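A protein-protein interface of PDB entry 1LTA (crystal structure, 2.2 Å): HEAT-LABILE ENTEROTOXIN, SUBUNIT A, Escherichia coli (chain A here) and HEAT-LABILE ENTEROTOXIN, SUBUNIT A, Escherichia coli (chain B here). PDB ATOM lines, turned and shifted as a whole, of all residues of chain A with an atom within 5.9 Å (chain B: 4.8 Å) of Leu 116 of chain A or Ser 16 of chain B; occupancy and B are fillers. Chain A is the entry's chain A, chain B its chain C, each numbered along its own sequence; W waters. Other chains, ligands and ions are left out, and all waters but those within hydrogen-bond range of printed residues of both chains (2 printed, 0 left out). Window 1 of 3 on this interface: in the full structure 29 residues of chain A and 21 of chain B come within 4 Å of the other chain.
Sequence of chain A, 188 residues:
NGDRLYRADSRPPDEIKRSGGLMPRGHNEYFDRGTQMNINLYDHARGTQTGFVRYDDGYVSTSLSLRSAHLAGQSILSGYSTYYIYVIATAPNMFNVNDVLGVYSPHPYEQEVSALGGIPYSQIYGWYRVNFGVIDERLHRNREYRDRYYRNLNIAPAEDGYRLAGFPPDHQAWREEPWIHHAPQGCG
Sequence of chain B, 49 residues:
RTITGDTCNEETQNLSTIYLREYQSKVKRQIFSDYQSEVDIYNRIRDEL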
ATOM      1  N   TYR A  30      -6.289 -19.414  -6.168  1.00  0.00           N
ATOM      2  CA  TYR A  30      -6.057 -20.049  -4.890  1.00  0.00           C
ATOM      3  C   TYR A  30      -5.685 -21.508  -5.034  1.00  0.00           C
ATOM      4  O   TYR A  30      -4.798 -22.020  -4.339  1.00  0.00           O
ATOM      5  CB  TYR A  30      -7.307 -19.950  -4.001  1.00  0.00           C
ATOM      6  CG  TYR A  30      -7.103 -20.486  -2.587  1.00  0.00           C
ATOM      7  CD1 TYR A  30      -6.140 -19.940  -1.755  1.00  0.00           C
ATOM      8  CD2 TYR A  30      -7.831 -21.558  -2.128  1.00  0.00           C
ATOM      9  CE1 TYR A  30      -5.896 -20.469  -0.485  1.00  0.00           C
ATOM     10  CE2 TYR A  30      -7.595 -22.090  -0.862  1.00  0.00           C
ATOM     11  CZ  TYR A  30      -6.624 -21.548  -0.043  1.00  0.00           C
ATOM     12  OH  TYR A  30      -6.372 -22.072   1.208  1.00  0.00           O
ATOM     13  N   MET A  37       5.114 -21.655  -5.459  1.00  0.00           N
ATOM     14  CA  MET A  37       5.373 -20.468  -4.663  1.00  0.00           C
ATOM     15  C   MET A  37       6.372 -20.719  -3.515  1.00  0.00           C
ATOM     16  O   MET A  37       6.357 -21.811  -2.929  1.00  0.00           O
ATOM     17  CB  MET A  37       3.945 -20.076  -4.248  1.00  0.00           C
ATOM     18  CG  MET A  37       3.669 -19.004  -3.230  1.00  0.00           C
ATOM     19  SD  MET A  37       1.896 -19.025  -2.900  1.00  0.00           S
ATOM     20  CE  MET A  37       1.705 -20.427  -1.848  1.00  0.00           C
ATOM     21  N   ILE A  39       7.153 -20.533   0.265  1.00  0.00           N
ATOM     22  CA  ILE A  39       6.329 -20.279   1.438  1.00  0.00           C
ATOM     23  C   ILE A  39       7.298 -20.327   2.585  1.00  0.00           C
ATOM     24  O   ILE A  39       7.836 -21.412   2.836  1.00  0.00           O
ATOM     25  CB  ILE A  39       5.255 -21.368   1.646  1.00  0.00           C
ATOM     26  CG1 ILE A  39       4.436 -21.566   0.385  1.00  0.00           C
ATOM     27  CG2 ILE A  39       4.306 -20.934   2.754  1.00  0.00           C
ATOM     28  CD1 ILE A  39       3.570 -22.828   0.470  1.00  0.00           C
ATOM     29  N   ASN A  40       7.556 -19.200   3.252  1.00  0.00           N
ATOM     30  CA  ASN A  40       8.465 -19.205   4.380  1.00  0.00           C
ATOM     31  C   ASN A  40       8.070 -18.120   5.352  1.00  0.00           C
ATOM     32  O   ASN A  40       8.216 -16.932   5.009  1.00  0.00           O
ATOM     33  CB  ASN A  40       9.918 -18.938   3.946  1.00  0.00           C
ATOM     34  CG  ASN A  40      10.927 -18.936   5.106  1.00  0.00           C
ATOM     35  OD1 ASN A  40      10.932 -18.105   6.014  1.00  0.00           O
ATOM     36  ND2 ASN A  40      11.838 -19.880   5.142  1.00  0.00           N
ATOM     37  N   GLY A  58       4.590 -16.429   0.351  1.00  0.00           N
ATOM     38  CA  GLY A  58       3.527 -17.381   0.585  1.00  0.00           C
ATOM     39  C   GLY A  58       2.499 -17.089   1.651  1.00  0.00           C
ATOM     40  O   GLY A  58       1.580 -17.878   1.836  1.00  0.00           O
ATOM     41  N   TYR A  59       2.572 -15.978   2.353  1.00  0.00           N
ATOM     42  CA  TYR A  59       1.604 -15.660   3.382  1.00  0.00           C
ATOM     43  C   TYR A  59       0.955 -14.327   3.070  1.00  0.00           C
ATOM     44  O   TYR A  59       1.599 -13.550   2.354  1.00  0.00           O
ATOM     45  CB  TYR A  59       2.306 -15.567   4.706  1.00  0.00           C
ATOM     46  CG  TYR A  59       2.773 -16.855   5.336  1.00  0.00           C
ATOM     47  CD1 TYR A  59       3.975 -17.433   4.977  1.00  0.00           C
ATOM     48  CD2 TYR A  59       1.976 -17.425   6.305  1.00  0.00           C
ATOM     49  CE1 TYR A  59       4.367 -18.595   5.606  1.00  0.00           C
ATOM     50  CE2 TYR A  59       2.374 -18.576   6.935  1.00  0.00           C
ATOM     51  CZ  TYR A  59       3.569 -19.162   6.584  1.00  0.00           C
ATOM     52  OH  TYR A  59       3.949 -20.341   7.236  1.00  0.00           O
ATOM     53  N   VAL A  60      -0.248 -14.002   3.587  1.00  0.00           N
ATOM     54  CA  VAL A  60      -0.880 -12.684   3.421  1.00  0.00           C
ATOM     55  C   VAL A  60      -1.133 -12.176   4.844  1.00  0.00           C
ATOM     56  O   VAL A  60      -1.739 -12.879   5.661  1.00  0.00           O
ATOM     57  CB  VAL A  60      -2.195 -12.821   2.643  1.00  0.00           C
ATOM     58  CG1 VAL A  60      -2.993 -11.526   2.549  1.00  0.00           C
ATOM     59  CG2 VAL A  60      -1.841 -13.108   1.209  1.00  0.00           C
ATOM     60  N   ASN A  93      -5.566 -21.665   8.910  1.00  0.00           N
ATOM     61  CA  ASN A  93      -4.561 -21.294   7.949  1.00  0.00           C
ATOM     62  C   ASN A  93      -3.884 -20.039   8.457  1.00  0.00           C
ATOM     63  O   ASN A  93      -2.989 -19.548   7.776  1.00  0.00           O
ATOM     64  CB  ASN A  93      -5.111 -20.941   6.534  1.00  0.00           C
ATOM     65  CG  ASN A  93      -6.260 -19.945   6.422  1.00  0.00           C
ATOM     66  OD1 ASN A  93      -6.934 -19.715   7.416  1.00  0.00           O
ATOM     67  ND2 ASN A  93      -6.663 -19.370   5.291  1.00  0.00           N
ATOM     68  N   MET A  94      -4.227 -19.477   9.616  1.00  0.00           N
ATOM     69  CA  MET A  94      -3.716 -18.197  10.068  1.00  0.00           C
ATOM     70  C   MET A  94      -2.739 -18.436  11.170  1.00  0.00           C
ATOM     71  O   MET A  94      -3.088 -19.257  12.016  1.00  0.00           O
ATOM     72  CB  MET A  94      -4.772 -17.345  10.680  1.00  0.00           C
ATOM     73  CG  MET A  94      -5.972 -17.001   9.861  1.00  0.00           C
ATOM     74  SD  MET A  94      -5.400 -15.769   8.700  1.00  0.00           S
ATOM     75  CE  MET A  94      -6.924 -15.576   7.862  1.00  0.00           C
ATOM     76  N   PHE A  95      -1.578 -17.767  11.279  1.00  0.00           N
ATOM     77  CA  PHE A  95      -0.663 -18.008  12.402  1.00  0.00           C
ATOM     78  C   PHE A  95      -0.297 -16.663  12.999  1.00  0.00           C
ATOM     79  O   PHE A  95      -0.107 -15.676  12.265  1.00  0.00           O
ATOM     80  CB  PHE A  95       0.663 -18.694  11.990  1.00  0.00           C
ATOM     81  CG  PHE A  95       0.480 -20.107  11.423  1.00  0.00           C
ATOM     82  CD1 PHE A  95       0.109 -20.293  10.094  1.00  0.00           C
ATOM     83  CD2 PHE A  95       0.631 -21.210  12.252  1.00  0.00           C
ATOM     84  CE1 PHE A  95      -0.112 -21.576   9.619  1.00  0.00           C
ATOM     85  CE2 PHE A  95       0.408 -22.489  11.759  1.00  0.00           C
ATOM     86  CZ  PHE A  95       0.038 -22.667  10.447  1.00  0.00           C
ATOM     87  N   SER A 114      -0.719 -14.097   9.974  1.00  0.00           N
ATOM     88  CA  SER A 114      -0.510 -14.291   8.543  1.00  0.00           C
ATOM     89  C   SER A 114      -1.157 -15.538   7.982  1.00  0.00           C
ATOM     90  O   SER A 114      -1.148 -16.575   8.643  1.00  0.00           O
ATOM     91  CB  SER A 114       0.952 -14.325   8.330  1.00  0.00           C
ATOM     92  OG  SER A 114       1.430 -12.998   8.391  1.00  0.00           O
ATOM     93  N   ALA A 115      -1.779 -15.440   6.814  1.00  0.00           N
ATOM     94  CA  ALA A 115      -2.487 -16.563   6.250  1.00  0.00           C
ATOM     95  C   ALA A 115      -1.559 -17.308   5.317  1.00  0.00           C
ATOM     96  O   ALA A 115      -1.083 -16.732   4.338  1.00  0.00           O
ATOM     97  CB  ALA A 115      -3.659 -16.117   5.437  1.00  0.00           C
ATOM     98  N   LEU A 116      -1.292 -18.573   5.624  1.00  0.00           N
ATOM     99  CA  LEU A 116      -0.479 -19.433   4.798  1.00  0.00           C
ATOM    100  C   LEU A 116      -1.218 -19.767   3.503  1.00  0.00           C
ATOM    101  O   LEU A 116      -2.259 -20.431   3.490  1.00  0.00           O
ATOM    102  CB  LEU A 116      -0.129 -20.683   5.620  1.00  0.00           C
ATOM    103  CG  LEU A 116       0.477 -22.045   5.111  1.00  0.00           C
ATOM    104  CD1 LEU A 116       1.067 -22.029   3.751  1.00  0.00           C
ATOM    105  CD2 LEU A 116       1.567 -22.409   6.109  1.00  0.00           C
ATOM    106  N   GLY A 117      -0.698 -19.276   2.379  1.00  0.00           N
ATOM    107  CA  GLY A 117      -1.252 -19.624   1.087  1.00  0.00           C
ATOM    108  C   GLY A 117      -2.285 -18.657   0.532  1.00  0.00           C
ATOM    109  O   GLY A 117      -2.711 -18.824  -0.629  1.00  0.00           O
ATOM    110  N   GLY A 118      -2.610 -17.614   1.326  1.00  0.00           N
ATOM    111  CA  GLY A 118      -3.596 -16.633   0.935  1.00  0.00           C
ATOM    112  C   GLY A 118      -4.878 -16.856   1.716  1.00  0.00           C
ATOM    113  O   GLY A 118      -4.898 -17.677   2.623  1.00  0.00           O
ATOM    114  N   LEU A 164       7.129 -24.752  10.883  1.00  0.00           N
ATOM    115  CA  LEU A 164       7.013 -24.004   9.648  1.00  0.00           C
ATOM    116  C   LEU A 164       7.639 -22.626   9.822  1.00  0.00           C
ATOM    117  O   LEU A 164       7.553 -21.823   8.890  1.00  0.00           O
ATOM    118  CB  LEU A 164       5.550 -23.789   9.235  1.00  0.00           C
ATOM    119  CG  LEU A 164       4.655 -24.998   9.257  1.00  0.00           C
ATOM    120  CD1 LEU A 164       3.264 -24.642   8.818  1.00  0.00           C
ATOM    121  CD2 LEU A 164       5.247 -26.041   8.359  1.00  0.00           C
ATOM    122  N   THR B  12      11.343 -27.028   4.981  1.00  0.00           N
ATOM    123  CA  THR B  12      10.429 -25.950   5.332  1.00  0.00           C
ATOM    124  C   THR B  12       9.407 -25.782   4.229  1.00  0.00           C
ATOM    125  O   THR B  12       8.198 -25.900   4.452  1.00  0.00           O
ATOM    126  CB  THR B  12      11.263 -24.658   5.553  1.00  0.00           C
ATOM    127  OG1 THR B  12      12.059 -24.873   6.730  1.00  0.00           O
ATOM    128  CG2 THR B  12      10.377 -23.411   5.617  1.00  0.00           C
ATOM    129  N   GLN B  13       9.902 -25.637   3.017  1.00  0.00           N
ATOM    130  CA  GLN B  13       9.046 -25.540   1.846  1.00  0.00           C
ATOM    131  C   GLN B  13       8.037 -26.684   1.740  1.00  0.00           C
ATOM    132  O   GLN B  13       6.829 -26.500   1.582  1.00  0.00           O
ATOM    133  CB  GLN B  13       9.944 -25.522   0.630  1.00  0.00           C
ATOM    134  CG  GLN B  13       9.288 -25.448  -0.735  1.00  0.00           C
ATOM    135  CD  GLN B  13       8.432 -24.206  -0.850  1.00  0.00           C
ATOM    136  OE1 GLN B  13       8.823 -23.109  -0.423  1.00  0.00           O
ATOM    137  NE2 GLN B  13       7.232 -24.364  -1.377  1.00  0.00           N
ATOM    138  N   ASN B  14       8.533 -27.889   1.891  1.00  0.00           N
ATOM    139  CA  ASN B  14       7.755 -29.089   1.698  1.00  0.00           C
ATOM    140  C   ASN B  14       6.700 -29.255   2.771  1.00  0.00           C
ATOM    141  O   ASN B  14       5.558 -29.593   2.485  1.00  0.00           O
ATOM    142  CB  ASN B  14       8.733 -30.256   1.661  1.00  0.00           C
ATOM    143  CG  ASN B  14       8.079 -31.638   1.640  1.00  0.00           C
ATOM    144  OD1 ASN B  14       7.460 -32.056   0.652  1.00  0.00           O
ATOM    145  ND2 ASN B  14       8.212 -32.423   2.718  1.00  0.00           N
ATOM    146  N   LEU B  15       7.016 -28.973   4.020  1.00  0.00           N
ATOM    147  CA  LEU B  15       6.060 -29.014   5.111  1.00  0.00           C
ATOM    148  C   LEU B  15       4.984 -27.914   5.041  1.00  0.00           C
ATOM    149  O   LEU B  15       3.826 -28.141   5.406  1.00  0.00           O
ATOM    150  CB  LEU B  15       6.844 -28.895   6.400  1.00  0.00           C
ATOM    151  CG  LEU B  15       7.627 -30.075   6.964  1.00  0.00           C
ATOM    152  CD1 LEU B  15       8.692 -29.637   7.963  1.00  0.00           C
ATOM    153  CD2 LEU B  15       6.604 -31.003   7.593  1.00  0.00           C
ATOM    154  N   SER B  16       5.335 -26.705   4.623  1.00  0.00           N
ATOM    155  CA  SER B  16       4.405 -25.628   4.457  1.00  0.00           C
ATOM    156  C   SER B  16       3.479 -25.977   3.321  1.00  0.00           C
ATOM    157  O   SER B  16       2.279 -25.705   3.417  1.00  0.00           O
ATOM    158  CB  SER B  16       5.153 -24.375   4.118  1.00  0.00           C
ATOM    159  OG  SER B  16       6.105 -24.074   5.110  1.00  0.00           O
ATOM    160  N   THR B  17       3.965 -26.550   2.229  1.00  0.00           N
ATOM    161  CA  THR B  17       3.078 -26.942   1.150  1.00  0.00           C
ATOM    162  C   THR B  17       2.117 -28.039   1.554  1.00  0.00           C
ATOM    163  O   THR B  17       0.953 -28.032   1.152  1.00  0.00           O
ATOM    164  CB  THR B  17       3.898 -27.389  -0.050  1.00  0.00           C
ATOM    165  OG1 THR B  17       4.621 -26.242  -0.473  1.00  0.00           O
ATOM    166  CG2 THR B  17       3.059 -27.858  -1.224  1.00  0.00           C
ATOM    167  N   ILE B  18       2.553 -28.972   2.381  1.00  0.00           N
ATOM    168  CA  ILE B  18       1.695 -30.037   2.861  1.00  0.00           C
ATOM    169  C   ILE B  18       0.604 -29.408   3.674  1.00  0.00           C
ATOM    170  O   ILE B  18      -0.564 -29.690   3.405  1.00  0.00           O
ATOM    171  CB  ILE B  18       2.510 -31.014   3.726  1.00  0.00           C
ATOM    172  CG1 ILE B  18       3.432 -31.807   2.799  1.00  0.00           C
ATOM    173  CG2 ILE B  18       1.594 -31.905   4.533  1.00  0.00           C
ATOM    174  CD1 ILE B  18       4.450 -32.688   3.533  1.00  0.00           C
ATOM    175  N   TYR B  19       1.012 -28.500   4.575  1.00  0.00           N
ATOM    176  CA  TYR B  19       0.083 -27.843   5.438  1.00  0.00           C
ATOM    177  C   TYR B  19      -0.924 -27.105   4.577  1.00  0.00           C
ATOM    178  O   TYR B  19      -2.139 -27.209   4.797  1.00  0.00           O
ATOM    179  CB  TYR B  19       0.822 -26.899   6.331  1.00  0.00           C
ATOM    180  CG  TYR B  19      -0.099 -26.485   7.449  1.00  0.00           C
ATOM    181  CD1 TYR B  19      -1.006 -25.463   7.275  1.00  0.00           C
ATOM    182  CD2 TYR B  19      -0.036 -27.116   8.653  1.00  0.00           C
ATOM    183  CE1 TYR B  19      -1.850 -25.061   8.281  1.00  0.00           C
ATOM    184  CE2 TYR B  19      -0.873 -26.723   9.677  1.00  0.00           C
ATOM    185  CZ  TYR B  19      -1.770 -25.694   9.481  1.00  0.00           C
ATOM    186  OH  TYR B  19      -2.583 -25.259  10.504  1.00  0.00           O
ATOM    187  N   LEU B  20      -0.487 -26.392   3.560  1.00  0.00           N
ATOM    188  CA  LEU B  20      -1.399 -25.710   2.680  1.00  0.00           C
ATOM    189  C   LEU B  20      -2.347 -26.653   1.939  1.00  0.00           C
ATOM    190  O   LEU B  20      -3.552 -26.371   1.977  1.00  0.00           O
ATOM    191  CB  LEU B  20      -0.600 -24.900   1.682  1.00  0.00           C
ATOM    192  CG  LEU B  20      -1.409 -24.228   0.593  1.00  0.00           C
ATOM    193  CD1 LEU B  20      -2.507 -23.364   1.173  1.00  0.00           C
ATOM    194  CD2 LEU B  20      -0.477 -23.368  -0.229  1.00  0.00           C
HETATM  195  O   HOH W   1       6.575 -21.473   6.447  1.00  0.00           O
HETATM  196  O   HOH W   2      10.573 -22.317   1.683  1.00  0.00           O
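O of Met 37 of chain A is in hydrogen-bond range of NE2 of Gln 13 of chain B, at 3.1 Å. The backbone NH (N) of Ile 39 of chain A lies within hydrogen-bond range of the side-chain amide oxygen (OE1) of Gln 13 of chain B (3.1 Å).
The backbone carbonyl oxygen (O) of Phe 95 of chain A sits at hydrogen-bond distance from the backbone NH (N) of Ser 114 of chain A. O of Asn 93 of chain A is in hydrogen-bond range of N of Leu 116 of chain A, at 2.9 Å. O of Gly 58 of chain A sits at hydrogen-bond distance from N of Gly 117 of chain A. The backbone carbonyl oxygen (O) of Gln 13 of chain B sits at hydrogen-bond distance from the side-chain hydroxyl (OG1) of Thr 17 of chain B, 3.0 Å away. The backbone carbonyl oxygen of Thr 12 of chain B sits at hydrogen-bond distance from the side-chain hydroxyl of Ser 16 of chain B, 2.9 Å away.
Among the printed residues, merely in contact across the chains: Phe 95 of chain A with Tyr 19 of chain B, Ile 39 of chain A with Thr 17 of chain B, Leu 116 of chain A with Leu 20 of chain B, Leu 164 of chain A with Ser 16 of chain B, Ile 39 of chain A with Ser 16 of chain B, Leu 164 of chain A with Leu 15 of chain B, Asn 40 of chain A with Thr 12 of chain B, Leu 116 of chain A with Ser 16 of chain B and Gly 117 of chain A with Leu 20 of chain B.
Leu 116 of chain A touches just these residues of chain B: Ser 16 and Leu 20. Ser 16 of chain B touches three residues of chain A. Of the printed residues of chain B, Leu 164 of chain A touches Leu 15 and Ser 16. Of the printed residues of chain A, Gln 13 of chain B touches Met 37 and Ile 39. Of the printed residues of chain A, Thr 12 of chain B touches Asn 40. Asn 14 of chain B touches none of the printed residues of chain A. Met 94 of chain A touches none of the printed residues of chain B. The nearest residue of chain B that does not touch Leu 116 of chain A is Tyr 19 of chain B (4.2 Å). The nearest residue of chain A that does not touch Ser 16 of chain B is Tyr 59 of chain A (4.8 Å). The nearest printed residue of chain B that does not touch Asn 40 of chain A is Ser 16 of chain B (5.4 Å).
Of the 9 printed residues of chain B, 7 touch a printed residue of chain A. Hydrophobic or aromatic side chains of chain B that line the printed part of chain A: Leu 15, Tyr 19 and Leu 20. Printed residues of chain A that touch a printed residue of chain B: Met 37, Ile 39, Asn 40, Phe 95, Leu 116, Gly 117 and Leu 164. Hydrophobic or aromatic side chains of chain A that line the printed part of chain B: Ile 39, Phe 95, Leu 116 and Leu 164. Along chain A the printed residues that touch a printed residue of chain B span positions 37 to 164. Among the printed residues, 11 pairs touch across the chains. Among the printed residues, no Asp or Glu carboxylate lies within 4 Å of a Lys or Arg side-chain nitrogen of the other chain.
Water W1 lies within hydrogen-bond range of O of Leu 164 of chain A, OG of Ser 16 of chain B and OH of Tyr 59 of chain A. Water W2 lies within hydrogen-bond range of the side-chain amide oxygen (OE1) of Gln 13 of chain B (2.9 Å) and the backbone carbonyl oxygen (O) of Ile 39 of chain A (3.1 Å).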
